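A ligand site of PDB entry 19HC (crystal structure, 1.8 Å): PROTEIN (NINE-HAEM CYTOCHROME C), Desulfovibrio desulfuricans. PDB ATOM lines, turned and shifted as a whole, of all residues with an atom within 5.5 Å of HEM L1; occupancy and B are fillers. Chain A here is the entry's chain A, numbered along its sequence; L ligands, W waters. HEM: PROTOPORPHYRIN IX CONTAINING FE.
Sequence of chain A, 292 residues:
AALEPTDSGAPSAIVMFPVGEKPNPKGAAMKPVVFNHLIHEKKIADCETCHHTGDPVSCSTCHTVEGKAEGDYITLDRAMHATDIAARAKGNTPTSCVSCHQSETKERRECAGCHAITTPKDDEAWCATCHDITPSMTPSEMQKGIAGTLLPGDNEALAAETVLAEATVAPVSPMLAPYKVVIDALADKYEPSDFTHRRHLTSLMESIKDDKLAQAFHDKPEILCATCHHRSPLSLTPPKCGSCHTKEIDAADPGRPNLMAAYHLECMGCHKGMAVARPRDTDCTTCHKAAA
A carbon (CAB) of HEM L1 is bonded to the side-chain sulfur (SG) of Cys 47 (1.8 Å). The side-chain sulfur (SG) of Cys 50 is covalently linked to a carbon (CAC) of HEM L1, 1.8 Å away. FE of HEM L1 is bound by NE2 of His 37 (2.0 Å). An iron atom (FE) of HEM L1 is bound by a ring nitrogen (NE2) of His 51 (2.0 Å). N of Ser 58 lies within hydrogen-bond range of O2A of HEM L1 (3.4 Å). A ring nitrogen (NE2) of His 40 binds an iron atom (FE) of HEM L2, at 2.0 Å. SG of Cys 59 is bonded to CAB of HEM L3, 1.8 Å away.
ND1 of His 37 is in hydrogen-bond range of OE1 of Glu 41 (2.8 Å). OG of Ser 60 is in hydrogen-bond range of OG of Ser 58, at 3.5 Å. The backbone NH of Phe 35 lies within hydrogen-bond range of the backbone carbonyl oxygen of Ile 14, 2.8 Å away. The backbone NH of Ala 10 sits at hydrogen-bond distance from the side-chain hydroxyl of Ser 8 (3.0 Å). OG of Ser 8 sits at hydrogen-bond distance from OE1 of Glu 41 (2.5 Å). O of Asp 46 lies within hydrogen-bond range of OG1 of Thr 49, 3.4 Å away.
Ser 8 touches HEM L1. Ala 10 touches HEM L1 (CB to C4A, 3.6 Å). Pro 11 touches HEM L1. CG1 of Ile 14 touches O2D of HEM L1, 3.7 Å away. CE of Met 16 touches O1D of HEM L1, at 3.6 Å. CE2 of Phe 35 touches C2D of HEM L1, at 3.5 Å. CD2 of His 40 touches CBC of HEM L1 (3.7 Å). CG2 of Ile 44 touches CMC of HEM L1 (3.6 Å). Asp 46 touches HEM L1. Pro 56 touches HEM L1 (O to CMA, 3.5 Å). Val 57 touches HEM L1. Cys 59 touches HEM L1 (N to CBD, 3.98 Å). Hydrophobic or aromatic side chains that line HEM L1: Ala 10, Pro 11, Ile 14, Met 16, Phe 35, His 37, His 40, Ile 44 and His 51. Within 4 Å of HEM L1: Ser 8, Ala 10, Pro 11, Ile 14, Met 16, Phe 35, His 37, His 40, Ile 44, Asp 46, Cys 47, Cys 50, His 51, Pro 56, Val 57, Ser 58 and Cys 59. The nearest printed residue that does not touch HEM L1 is Ser 60 (4.2 Å).
Water W2 lies within hydrogen-bond range of O1D of HEM L1 (2.4 Å), N of Ser 60 (2.7 Å) and N of Cys 59 (3.3 Å). Water W1 bridges an oxygen (O1D) of HEM L1 (2.4 Å) and the side-chain hydroxyl of Ser 60 (2.8 Å). Water W5 lies within hydrogen-bond range of O2A of HEM L1 (2.5 Å) and N of Ser 58 (3.1 Å). Water W4 lies within hydrogen-bond range of an oxygen (O2D) of HEM L1 (2.5 Å) and the backbone carbonyl oxygen (O) of Val 15 (2.8 Å). Water W3 lies within hydrogen-bond range of O2A of HEM L1 (2.9 Å) and O of Pro 56 (3.2 Å).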
ATOM      1  N   SER A   8       6.821 -16.872 -14.556  1.00  0.00           N
ATOM      2  CA  SER A   8       7.576 -17.623 -15.533  1.00  0.00           C
ATOM      3  C   SER A   8       7.243 -19.118 -15.583  1.00  0.00           C
ATOM      4  O   SER A   8       7.481 -19.732 -16.642  1.00  0.00           O
ATOM      5  CB  SER A   8       9.079 -17.482 -15.246  1.00  0.00           C
ATOM      6  OG  SER A   8       9.419 -18.066 -13.998  1.00  0.00           O
ATOM      7  N   GLY A   9       6.854 -19.734 -14.483  1.00  0.00           N
ATOM      8  CA  GLY A   9       6.746 -21.186 -14.423  1.00  0.00           C
ATOM      9  C   GLY A   9       8.016 -21.815 -13.877  1.00  0.00           C
ATOM     10  O   GLY A   9       8.098 -23.039 -13.733  1.00  0.00           O
ATOM     11  N   ALA A  10       9.076 -21.022 -13.626  1.00  0.00           N
ATOM     12  CA  ALA A  10      10.239 -21.515 -12.876  1.00  0.00           C
ATOM     13  C   ALA A  10       9.800 -21.695 -11.421  1.00  0.00           C
ATOM     14  O   ALA A  10       8.802 -21.119 -10.968  1.00  0.00           O
ATOM     15  CB  ALA A  10      11.366 -20.445 -12.847  1.00  0.00           C
ATOM     16  N   PRO A  11      10.552 -22.500 -10.669  1.00  0.00           N
ATOM     17  CA  PRO A  11      10.233 -22.696  -9.265  1.00  0.00           C
ATOM     18  C   PRO A  11      10.417 -21.340  -8.568  1.00  0.00           C
ATOM     19  O   PRO A  11      11.253 -20.591  -9.055  1.00  0.00           O
ATOM     20  CB  PRO A  11      11.266 -23.719  -8.786  1.00  0.00           C
ATOM     21  CG  PRO A  11      12.330 -23.744  -9.827  1.00  0.00           C
ATOM     22  CD  PRO A  11      11.752 -23.220 -11.101  1.00  0.00           C
ATOM     23  N   ILE A  14      14.571 -22.397  -5.441  1.00  0.00           N
ATOM     24  CA  ILE A  14      15.085 -23.710  -5.823  1.00  0.00           C
ATOM     25  C   ILE A  14      16.433 -23.961  -5.142  1.00  0.00           C
ATOM     26  O   ILE A  14      17.326 -23.099  -5.128  1.00  0.00           O
ATOM     27  CB  ILE A  14      15.265 -23.831  -7.335  1.00  0.00           C
ATOM     28  CG1 ILE A  14      15.778 -25.218  -7.787  1.00  0.00           C
ATOM     29  CG2 ILE A  14      16.153 -22.748  -7.904  1.00  0.00           C
ATOM     30  N   VAL A  15      16.560 -25.185  -4.644  1.00  0.00           N
ATOM     31  CA  VAL A  15      17.883 -25.555  -4.113  1.00  0.00           C
ATOM     32  C   VAL A  15      18.777 -26.016  -5.273  1.00  0.00           C
ATOM     33  O   VAL A  15      18.330 -26.879  -6.037  1.00  0.00           O
ATOM     34  CB  VAL A  15      17.776 -26.708  -3.115  1.00  0.00           C
ATOM     35  CG1 VAL A  15      19.139 -26.905  -2.469  1.00  0.00           C
ATOM     36  CG2 VAL A  15      16.665 -26.456  -2.114  1.00  0.00           C
ATOM     37  N   MET A  16      19.963 -25.466  -5.372  1.00  0.00           N
ATOM     38  CA  MET A  16      20.981 -25.699  -6.381  1.00  0.00           C
ATOM     39  C   MET A  16      22.087 -26.521  -5.737  1.00  0.00           C
ATOM     40  O   MET A  16      22.604 -26.026  -4.723  1.00  0.00           O
ATOM     41  CB  MET A  16      21.623 -24.374  -6.882  1.00  0.00           C
ATOM     42  CG  MET A  16      20.554 -23.490  -7.515  1.00  0.00           C
ATOM     43  SD  MET A  16      21.164 -21.896  -8.090  1.00  0.00           S
ATOM     44  CE  MET A  16      22.294 -22.397  -9.372  1.00  0.00           C
ATOM     45  N   PHE A  35      18.197 -20.507  -4.344  1.00  0.00           N
ATOM     46  CA  PHE A  35      18.055 -19.326  -5.186  1.00  0.00           C
ATOM     47  C   PHE A  35      16.604 -18.880  -5.287  1.00  0.00           C
ATOM     48  O   PHE A  35      15.748 -19.719  -5.536  1.00  0.00           O
ATOM     49  CB  PHE A  35      18.571 -19.686  -6.569  1.00  0.00           C
ATOM     50  CG  PHE A  35      18.406 -18.598  -7.607  1.00  0.00           C
ATOM     51  CD1 PHE A  35      19.215 -17.454  -7.546  1.00  0.00           C
ATOM     52  CD2 PHE A  35      17.486 -18.719  -8.636  1.00  0.00           C
ATOM     53  CE1 PHE A  35      19.121 -16.510  -8.552  1.00  0.00           C
ATOM     54  CE2 PHE A  35      17.419 -17.798  -9.656  1.00  0.00           C
ATOM     55  CZ  PHE A  35      18.200 -16.638  -9.589  1.00  0.00           C
ATOM     56  N   HIS A  37      14.198 -17.463  -7.226  1.00  0.00           N
ATOM     57  CA  HIS A  37      13.929 -17.123  -8.621  1.00  0.00           C
ATOM     58  C   HIS A  37      12.845 -16.058  -8.731  1.00  0.00           C
ATOM     59  O   HIS A  37      12.867 -15.193  -9.625  1.00  0.00           O
ATOM     60  CB  HIS A  37      13.488 -18.404  -9.380  1.00  0.00           C
ATOM     61  CG  HIS A  37      13.652 -18.254 -10.854  1.00  0.00           C
ATOM     62  ND1 HIS A  37      12.860 -17.485 -11.675  1.00  0.00           N
ATOM     63  CD2 HIS A  37      14.609 -18.815 -11.647  1.00  0.00           C
ATOM     64  CE1 HIS A  37      13.314 -17.601 -12.913  1.00  0.00           C
ATOM     65  NE2 HIS A  37      14.362 -18.400 -12.933  1.00  0.00           N
ATOM     66  N   HIS A  40      14.322 -12.682  -8.246  1.00  0.00           N
ATOM     67  CA  HIS A  40      15.176 -12.289  -9.366  1.00  0.00           C
ATOM     68  C   HIS A  40      14.407 -12.010 -10.643  1.00  0.00           C
ATOM     69  O   HIS A  40      14.723 -11.067 -11.365  1.00  0.00           O
ATOM     70  CB  HIS A  40      16.265 -13.328  -9.622  1.00  0.00           C
ATOM     71  CG  HIS A  40      17.377 -13.318  -8.622  1.00  0.00           C
ATOM     72  ND1 HIS A  40      17.348 -13.883  -7.371  1.00  0.00           N
ATOM     73  CD2 HIS A  40      18.596 -12.722  -8.767  1.00  0.00           C
ATOM     74  CE1 HIS A  40      18.528 -13.648  -6.782  1.00  0.00           C
ATOM     75  NE2 HIS A  40      19.301 -12.938  -7.601  1.00  0.00           N
ATOM     76  N   GLU A  41      13.407 -12.845 -10.974  1.00  0.00           N
ATOM     77  CA  GLU A  41      12.750 -12.566 -12.256  1.00  0.00           C
ATOM     78  C   GLU A  41      11.882 -11.318 -12.164  1.00  0.00           C
ATOM     79  O   GLU A  41      11.569 -10.683 -13.186  1.00  0.00           O
ATOM     80  CB  GLU A  41      11.962 -13.788 -12.757  1.00  0.00           C
ATOM     81  CG  GLU A  41      10.707 -14.069 -11.957  1.00  0.00           C
ATOM     82  CD  GLU A  41       9.942 -15.247 -12.545  1.00  0.00           C
ATOM     83  OE1 GLU A  41      10.431 -16.404 -12.482  1.00  0.00           O
ATOM     84  OE2 GLU A  41       8.879 -15.001 -13.158  1.00  0.00           O
ATOM     85  N   ILE A  44      14.936  -8.566 -12.827  1.00  0.00           N
ATOM     86  CA  ILE A  44      15.712  -8.690 -14.049  1.00  0.00           C
ATOM     87  C   ILE A  44      14.745  -9.116 -15.151  1.00  0.00           C
ATOM     88  O   ILE A  44      14.268 -10.248 -15.164  1.00  0.00           O
ATOM     89  CB  ILE A  44      16.849  -9.684 -13.866  1.00  0.00           C
ATOM     90  CG1 ILE A  44      17.768  -9.414 -12.666  1.00  0.00           C
ATOM     91  CG2 ILE A  44      17.675  -9.891 -15.120  1.00  0.00           C
ATOM     92  CD1 ILE A  44      18.441  -8.056 -12.754  1.00  0.00           C
ATOM     93  N   ALA A  45      14.472  -8.223 -16.076  1.00  0.00           N
ATOM     94  CA  ALA A  45      13.380  -8.431 -17.031  1.00  0.00           C
ATOM     95  C   ALA A  45      13.652  -9.458 -18.098  1.00  0.00           C
ATOM     96  O   ALA A  45      12.745 -10.027 -18.708  1.00  0.00           O
ATOM     97  CB  ALA A  45      13.070  -7.076 -17.677  1.00  0.00           C
ATOM     98  N   ASP A  46      14.927  -9.660 -18.443  1.00  0.00           N
ATOM     99  CA  ASP A  46      15.177 -10.499 -19.606  1.00  0.00           C
ATOM    100  C   ASP A  46      15.593 -11.889 -19.152  1.00  0.00           C
ATOM    101  O   ASP A  46      16.625 -11.976 -18.493  1.00  0.00           O
ATOM    102  CB  ASP A  46      16.240  -9.800 -20.460  1.00  0.00           C
ATOM    103  CG  ASP A  46      16.649 -10.510 -21.725  1.00  0.00           C
ATOM    104  OD1 ASP A  46      16.300 -11.692 -21.920  1.00  0.00           O
ATOM    105  OD2 ASP A  46      17.301  -9.831 -22.564  1.00  0.00           O
ATOM    106  N   CYS A  47      14.855 -12.946 -19.532  1.00  0.00           N
ATOM    107  CA  CYS A  47      15.242 -14.262 -19.045  1.00  0.00           C
ATOM    108  C   CYS A  47      16.643 -14.646 -19.502  1.00  0.00           C
ATOM    109  O   CYS A  47      17.338 -15.386 -18.789  1.00  0.00           O
ATOM    110  CB  CYS A  47      14.315 -15.352 -19.603  1.00  0.00           C
ATOM    111  SG  CYS A  47      12.576 -15.035 -19.287  1.00  0.00           S
ATOM    112  N   THR A  49      19.217 -12.909 -19.969  1.00  0.00           N
ATOM    113  CA  THR A  49      20.372 -12.287 -19.327  1.00  0.00           C
ATOM    114  C   THR A  49      21.112 -13.367 -18.555  1.00  0.00           C
ATOM    115  O   THR A  49      22.327 -13.500 -18.530  1.00  0.00           O
ATOM    116  CB  THR A  49      19.947 -11.164 -18.363  1.00  0.00           C
ATOM    117  OG1 THR A  49      19.391 -10.085 -19.100  1.00  0.00           O
ATOM    118  CG2 THR A  49      21.150 -10.638 -17.584  1.00  0.00           C
ATOM    119  N   CYS A  50      20.296 -14.194 -17.882  1.00  0.00           N
ATOM    120  CA  CYS A  50      20.914 -15.260 -17.103  1.00  0.00           C
ATOM    121  C   CYS A  50      21.003 -16.548 -17.883  1.00  0.00           C
ATOM    122  O   CYS A  50      22.046 -17.207 -17.922  1.00  0.00           O
ATOM    123  CB  CYS A  50      20.041 -15.511 -15.844  1.00  0.00           C
ATOM    124  SG  CYS A  50      20.032 -14.044 -14.783  1.00  0.00           S
ATOM    125  N   HIS A  51      19.861 -16.961 -18.440  1.00  0.00           N
ATOM    126  CA  HIS A  51      19.864 -18.216 -19.201  1.00  0.00           C
ATOM    127  C   HIS A  51      20.431 -17.898 -20.590  1.00  0.00           C
ATOM    128  O   HIS A  51      19.653 -17.752 -21.533  1.00  0.00           O
ATOM    129  CB  HIS A  51      18.420 -18.728 -19.323  1.00  0.00           C
ATOM    130  CG  HIS A  51      17.785 -19.052 -17.997  1.00  0.00           C
ATOM    131  ND1 HIS A  51      18.089 -20.221 -17.341  1.00  0.00           N
ATOM    132  CD2 HIS A  51      16.883 -18.402 -17.213  1.00  0.00           C
ATOM    133  CE1 HIS A  51      17.441 -20.269 -16.181  1.00  0.00           C
ATOM    134  NE2 HIS A  51      16.708 -19.170 -16.088  1.00  0.00           N
ATOM    135  N   PRO A  56      15.672 -22.572 -21.090  1.00  0.00           N
ATOM    136  CA  PRO A  56      15.194 -22.483 -19.692  1.00  0.00           C
ATOM    137  C   PRO A  56      15.464 -23.734 -18.857  1.00  0.00           C
ATOM    138  O   PRO A  56      14.556 -24.461 -18.419  1.00  0.00           O
ATOM    139  CB  PRO A  56      13.685 -22.323 -19.915  1.00  0.00           C
ATOM    140  CG  PRO A  56      13.423 -23.139 -21.157  1.00  0.00           C
ATOM    141  CD  PRO A  56      14.611 -22.888 -22.056  1.00  0.00           C
ATOM    142  N   VAL A  57      16.733 -24.044 -18.606  1.00  0.00           N
ATOM    143  CA  VAL A  57      17.178 -25.247 -17.911  1.00  0.00           C
ATOM    144  C   VAL A  57      18.210 -24.861 -16.830  1.00  0.00           C
ATOM    145  O   VAL A  57      18.743 -23.751 -16.918  1.00  0.00           O
ATOM    146  CB  VAL A  57      17.914 -26.215 -18.869  1.00  0.00           C
ATOM    147  CG1 VAL A  57      16.945 -26.752 -19.909  1.00  0.00           C
ATOM    148  CG2 VAL A  57      19.063 -25.477 -19.549  1.00  0.00           C
ATOM    149  N   SER A  58      18.447 -25.774 -15.918  1.00  0.00           N
ATOM    150  CA  SER A  58      19.439 -25.606 -14.857  1.00  0.00           C
ATOM    151  C   SER A  58      20.813 -25.372 -15.459  1.00  0.00           C
ATOM    152  O   SER A  58      21.233 -26.088 -16.384  1.00  0.00           O
ATOM    153  CB  SER A  58      19.484 -26.828 -13.938  1.00  0.00           C
ATOM    154  OG  SER A  58      20.021 -27.962 -14.572  1.00  0.00           O
ATOM    155  N   CYS A  59      21.513 -24.363 -14.922  1.00  0.00           N
ATOM    156  CA  CYS A  59      22.894 -24.115 -15.373  1.00  0.00           C
ATOM    157  C   CYS A  59      23.718 -25.385 -15.257  1.00  0.00           C
ATOM    158  O   CYS A  59      24.600 -25.612 -16.108  1.00  0.00           O
ATOM    159  CB  CYS A  59      23.582 -23.074 -14.470  1.00  0.00           C
ATOM    160  SG  CYS A  59      22.564 -21.637 -14.113  1.00  0.00           S
ATOM    161  N   SER A  60      23.513 -26.214 -14.239  1.00  0.00           N
ATOM    162  CA  SER A  60      24.356 -27.398 -14.072  1.00  0.00           C
ATOM    163  C   SER A  60      24.084 -28.488 -15.113  1.00  0.00           C
ATOM    164  O   SER A  60      24.888 -29.418 -15.171  1.00  0.00           O
ATOM    165  CB  SER A  60      24.176 -28.077 -12.693  1.00  0.00           C
ATOM    166  OG  SER A  60      22.793 -28.279 -12.477  1.00  0.00           O
HETATM  167  CHA HEM L   1      16.051 -21.892 -13.139  1.00  0.00           C
HETATM  168  CHB HEM L   1      13.005 -20.063 -16.405  1.00  0.00           C
HETATM  169  CHC HEM L   1      14.689 -15.609 -15.519  1.00  0.00           C
HETATM  170  CHD HEM L   1      18.417 -17.648 -13.121  1.00  0.00           C
HETATM  171  C1A HEM L   1      14.994 -21.765 -14.034  1.00  0.00           C
HETATM  172  C2A HEM L   1      14.046 -22.789 -14.400  1.00  0.00           C
HETATM  173  C3A HEM L   1      13.310 -22.344 -15.414  1.00  0.00           C
HETATM  174  C4A HEM L   1      13.656 -20.945 -15.582  1.00  0.00           C
HETATM  175  CMA HEM L   1      12.214 -23.070 -16.249  1.00  0.00           C
HETATM  176  CAA HEM L   1      14.147 -24.244 -13.866  1.00  0.00           C
HETATM  177  CBA HEM L   1      15.076 -25.051 -14.790  1.00  0.00           C
HETATM  178  CGA HEM L   1      15.261 -26.512 -14.459  1.00  0.00           C
HETATM  179  O1A HEM L   1      15.150 -26.777 -13.242  1.00  0.00           O
HETATM  180  O2A HEM L   1      15.431 -27.310 -15.414  1.00  0.00           O
HETATM  181  C1B HEM L   1      13.179 -18.691 -16.428  1.00  0.00           C
HETATM  182  C2B HEM L   1      12.467 -17.780 -17.296  1.00  0.00           C
HETATM  183  C3B HEM L   1      12.943 -16.546 -17.061  1.00  0.00           C
HETATM  184  C4B HEM L   1      13.994 -16.682 -16.062  1.00  0.00           C
HETATM  185  CMB HEM L   1      11.233 -18.195 -18.144  1.00  0.00           C
HETATM  186  CAB HEM L   1      12.334 -15.202 -17.494  1.00  0.00           C
HETATM  187  CBB HEM L   1      11.069 -14.850 -17.107  1.00  0.00           C
HETATM  188  C1C HEM L   1      15.914 -15.804 -14.846  1.00  0.00           C
HETATM  189  C2C HEM L   1      16.809 -14.727 -14.461  1.00  0.00           C
HETATM  190  C3C HEM L   1      17.783 -15.261 -13.714  1.00  0.00           C
HETATM  191  C4C HEM L   1      17.611 -16.707 -13.748  1.00  0.00           C
HETATM  192  CMC HEM L   1      16.531 -13.245 -14.755  1.00  0.00           C
HETATM  193  CAC HEM L   1      19.119 -14.594 -13.272  1.00  0.00           C
HETATM  194  CBC HEM L   1      18.995 -13.567 -12.357  1.00  0.00           C
HETATM  195  C1D HEM L   1      18.109 -18.991 -12.935  1.00  0.00           C
HETATM  196  C2D HEM L   1      18.811 -19.916 -12.064  1.00  0.00           C
HETATM  197  C3D HEM L   1      18.116 -21.040 -12.001  1.00  0.00           C
HETATM  198  C4D HEM L   1      16.946 -20.884 -12.861  1.00  0.00           C
HETATM  199  CMD HEM L   1      20.152 -19.542 -11.358  1.00  0.00           C
HETATM  200  CAD HEM L   1      18.332 -22.354 -11.202  1.00  0.00           C
HETATM  201  CBD HEM L   1      19.004 -23.507 -11.948  1.00  0.00           C
HETATM  202  CGD HEM L   1      19.362 -24.681 -11.028  1.00  0.00           C
HETATM  203  O1D HEM L   1      20.539 -25.062 -11.051  1.00  0.00           O
HETATM  204  O2D HEM L   1      18.428 -25.103 -10.310  1.00  0.00           O
HETATM  205  NA  HEM L   1      14.708 -20.607 -14.745  1.00  0.00           N
HETATM  206  NB  HEM L   1      14.156 -18.001 -15.731  1.00  0.00           N
HETATM  207  NC  HEM L   1      16.352 -16.986 -14.309  1.00  0.00           N
HETATM  208  ND  HEM L   1      16.920 -19.594 -13.342  1.00  0.00           N
HETATM  209 FE   HEM L   1      15.519 -18.795 -14.510  1.00  0.00          FE
HETATM  210  CHA HEM L   2      19.450 -10.440  -4.893  1.00  0.00           C
HETATM  211  CHB HEM L   2      21.805 -14.666  -4.889  1.00  0.00           C
HETATM  212  CHC HEM L   2      22.375 -14.226  -9.628  1.00  0.00           C
HETATM  213  CHD HEM L   2      20.818  -9.681  -9.490  1.00  0.00           C
HETATM  214  C1A HEM L   2      20.095 -11.566  -4.454  1.00  0.00           C
HETATM  215  C2A HEM L   2      19.997 -12.109  -3.114  1.00  0.00           C
HETATM  216  C3A HEM L   2      20.737 -13.216  -3.092  1.00  0.00           C
HETATM  217  C4A HEM L   2      21.160 -13.506  -4.448  1.00  0.00           C
HETATM  218  CMA HEM L   2      21.000 -14.153  -1.902  1.00  0.00           C
HETATM  219  CAA HEM L   2      19.168 -11.419  -2.000  1.00  0.00           C
HETATM  220  CBA HEM L   2      17.661 -11.747  -2.047  1.00  0.00           C
HETATM  221  CGA HEM L   2      17.384 -13.229  -2.207  1.00  0.00           C
HETATM  222  O1A HEM L   2      17.401 -13.853  -1.133  1.00  0.00           O
HETATM  223  O2A HEM L   2      17.249 -13.700  -3.353  1.00  0.00           O
HETATM  224  C1B HEM L   2      22.104 -14.954  -6.206  1.00  0.00           C
HETATM  225  C2B HEM L   2      22.546 -16.235  -6.725  1.00  0.00           C
HETATM  226  C3B HEM L   2      22.706 -16.133  -8.036  1.00  0.00           C
HETATM  227  C4B HEM L   2      22.251 -14.800  -8.383  1.00  0.00           C
HETATM  228  CMB HEM L   2      22.890 -17.466  -5.843  1.00  0.00           C
HETATM  229  CAB HEM L   2      23.246 -17.179  -9.059  1.00  0.00           C
HETATM  230  CBB HEM L   2      22.675 -18.444  -9.000  1.00  0.00           C
HETATM  231  C1C HEM L   2      22.169 -12.899  -9.971  1.00  0.00           C
HETATM  232  C2C HEM L   2      22.239 -12.398 -11.331  1.00  0.00           C
HETATM  233  C3C HEM L   2      21.751 -11.153 -11.325  1.00  0.00           C
HETATM  234  C4C HEM L   2      21.430 -10.839  -9.937  1.00  0.00           C
HETATM  235  CMC HEM L   2      22.938 -13.208 -12.438  1.00  0.00           C
HETATM  236  CAC HEM L   2      21.840 -10.090 -12.461  1.00  0.00           C
HETATM  237  CBC HEM L   2      21.674 -10.474 -13.755  1.00  0.00           C
HETATM  238  C1D HEM L   2      20.305  -9.510  -8.217  1.00  0.00           C
HETATM  239  C2D HEM L   2      19.487  -8.372  -7.806  1.00  0.00           C
HETATM  240  C3D HEM L   2      19.066  -8.604  -6.557  1.00  0.00           C
HETATM  241  C4D HEM L   2      19.511  -9.914  -6.172  1.00  0.00           C
HETATM  242  CMD HEM L   2      19.134  -7.183  -8.713  1.00  0.00           C
HETATM  243  CAD HEM L   2      18.078  -7.737  -5.760  1.00  0.00           C
HETATM  244  CBD HEM L   2      16.590  -8.069  -6.023  1.00  0.00           C
HETATM  245  CGD HEM L   2      15.629  -7.031  -5.499  1.00  0.00           C
HETATM  246  O1D HEM L   2      14.413  -7.327  -5.459  1.00  0.00           O
HETATM  247  O2D HEM L   2      16.128  -5.910  -5.223  1.00  0.00           O
HETATM  248  NA  HEM L   2      20.768 -12.468  -5.267  1.00  0.00           N
HETATM  249  NB  HEM L   2      21.890 -14.085  -7.261  1.00  0.00           N
HETATM  250  NC  HEM L   2      21.528 -11.977  -9.158  1.00  0.00           N
HETATM  251  ND  HEM L   2      20.340 -10.407  -7.169  1.00  0.00           N
HETATM  252 FE   HEM L   2      21.131 -12.236  -7.216  1.00  0.00          FE
HETATM  253  CHA HEM L   3      29.676 -19.681 -20.582  1.00  0.00           C
HETATM  254  CHB HEM L   3      26.996 -18.898 -16.602  1.00  0.00           C
HETATM  255  CHC HEM L   3      23.661 -22.031 -18.211  1.00  0.00           C
HETATM  256  CHD HEM L   3      26.710 -23.330 -21.733  1.00  0.00           C
HETATM  257  C1A HEM L   3      29.221 -19.225 -19.355  1.00  0.00           C
HETATM  258  C2A HEM L   3      29.913 -18.252 -18.546  1.00  0.00           C
HETATM  259  C3A HEM L   3      29.245 -18.108 -17.395  1.00  0.00           C
HETATM  260  C4A HEM L   3      28.010 -18.879 -17.523  1.00  0.00           C
HETATM  261  CMA HEM L   3      29.456 -16.987 -16.355  1.00  0.00           C
HETATM  262  CAA HEM L   3      31.170 -17.481 -19.005  1.00  0.00           C
HETATM  263  CBA HEM L   3      32.477 -18.048 -18.449  1.00  0.00           C
HETATM  264  CGA HEM L   3      33.719 -17.316 -18.874  1.00  0.00           C
HETATM  265  O1A HEM L   3      33.696 -16.561 -19.878  1.00  0.00           O
HETATM  266  O2A HEM L   3      34.722 -17.563 -18.166  1.00  0.00           O
HETATM  267  C1B HEM L   3      25.845 -19.673 -16.722  1.00  0.00           C
HETATM  268  C2B HEM L   3      24.757 -19.665 -15.776  1.00  0.00           C
HETATM  269  C3B HEM L   3      23.774 -20.431 -16.266  1.00  0.00           C
HETATM  270  C4B HEM L   3      24.253 -20.954 -17.547  1.00  0.00           C
HETATM  271  CMB HEM L   3      24.731 -18.762 -14.510  1.00  0.00           C
HETATM  272  CAB HEM L   3      22.375 -20.706 -15.672  1.00  0.00           C
HETATM  273  CBB HEM L   3      21.526 -19.648 -15.497  1.00  0.00           C
HETATM  274  C1C HEM L   3      24.192 -22.614 -19.350  1.00  0.00           C
HETATM  275  C2C HEM L   3      23.536 -23.632 -20.167  1.00  0.00           C
HETATM  276  C3C HEM L   3      24.512 -24.206 -20.921  1.00  0.00           C
HETATM  277  C4C HEM L   3      25.654 -23.334 -20.860  1.00  0.00           C
HETATM  278  CMC HEM L   3      22.250 -24.343 -19.673  1.00  0.00           C
HETATM  279  CAC HEM L   3      24.325 -25.377 -21.929  1.00  0.00           C
HETATM  280  CBC HEM L   3      23.223 -25.329 -22.737  1.00  0.00           C
HETATM  281  C1D HEM L   3      27.791 -22.477 -21.707  1.00  0.00           C
HETATM  282  C2D HEM L   3      28.860 -22.437 -22.701  1.00  0.00           C
HETATM  283  C3D HEM L   3      29.536 -21.307 -22.504  1.00  0.00           C
HETATM  284  C4D HEM L   3      29.062 -20.722 -21.263  1.00  0.00           C
HETATM  285  CMD HEM L   3      28.813 -23.329 -23.971  1.00  0.00           C
HETATM  286  CAD HEM L   3      30.506 -20.565 -23.453  1.00  0.00           C
HETATM  287  CBD HEM L   3      29.911 -19.417 -24.285  1.00  0.00           C
HETATM  288  CGD HEM L   3      30.968 -18.491 -24.839  1.00  0.00           C
HETATM  289  O1D HEM L   3      30.585 -17.510 -25.520  1.00  0.00           O
HETATM  290  O2D HEM L   3      32.149 -18.800 -24.530  1.00  0.00           O
HETATM  291  NA  HEM L   3      28.081 -19.631 -18.682  1.00  0.00           N
HETATM  292  NB  HEM L   3      25.518 -20.472 -17.810  1.00  0.00           N
HETATM  293  NC  HEM L   3      25.411 -22.321 -19.923  1.00  0.00           N
HETATM  294  ND  HEM L   3      27.985 -21.453 -20.798  1.00  0.00           N
HETATM  295 FE   HEM L   3      26.749 -20.987 -19.306  1.00  0.00          FE
HETATM  296  O   HOH W   1      21.542 -27.098 -10.262  1.00  0.00           O
HETATM  297  O   HOH W   2      22.776 -24.984 -11.919  1.00  0.00           O
HETATM  298  O   HOH W   3      13.858 -27.495 -17.833  1.00  0.00           O
HETATM  299  O   HOH W   4      18.310 -27.132  -8.793  1.00  0.00           O
HETATM  300  O   HOH W   5      17.386 -28.625 -16.232  1.00  0.00           O
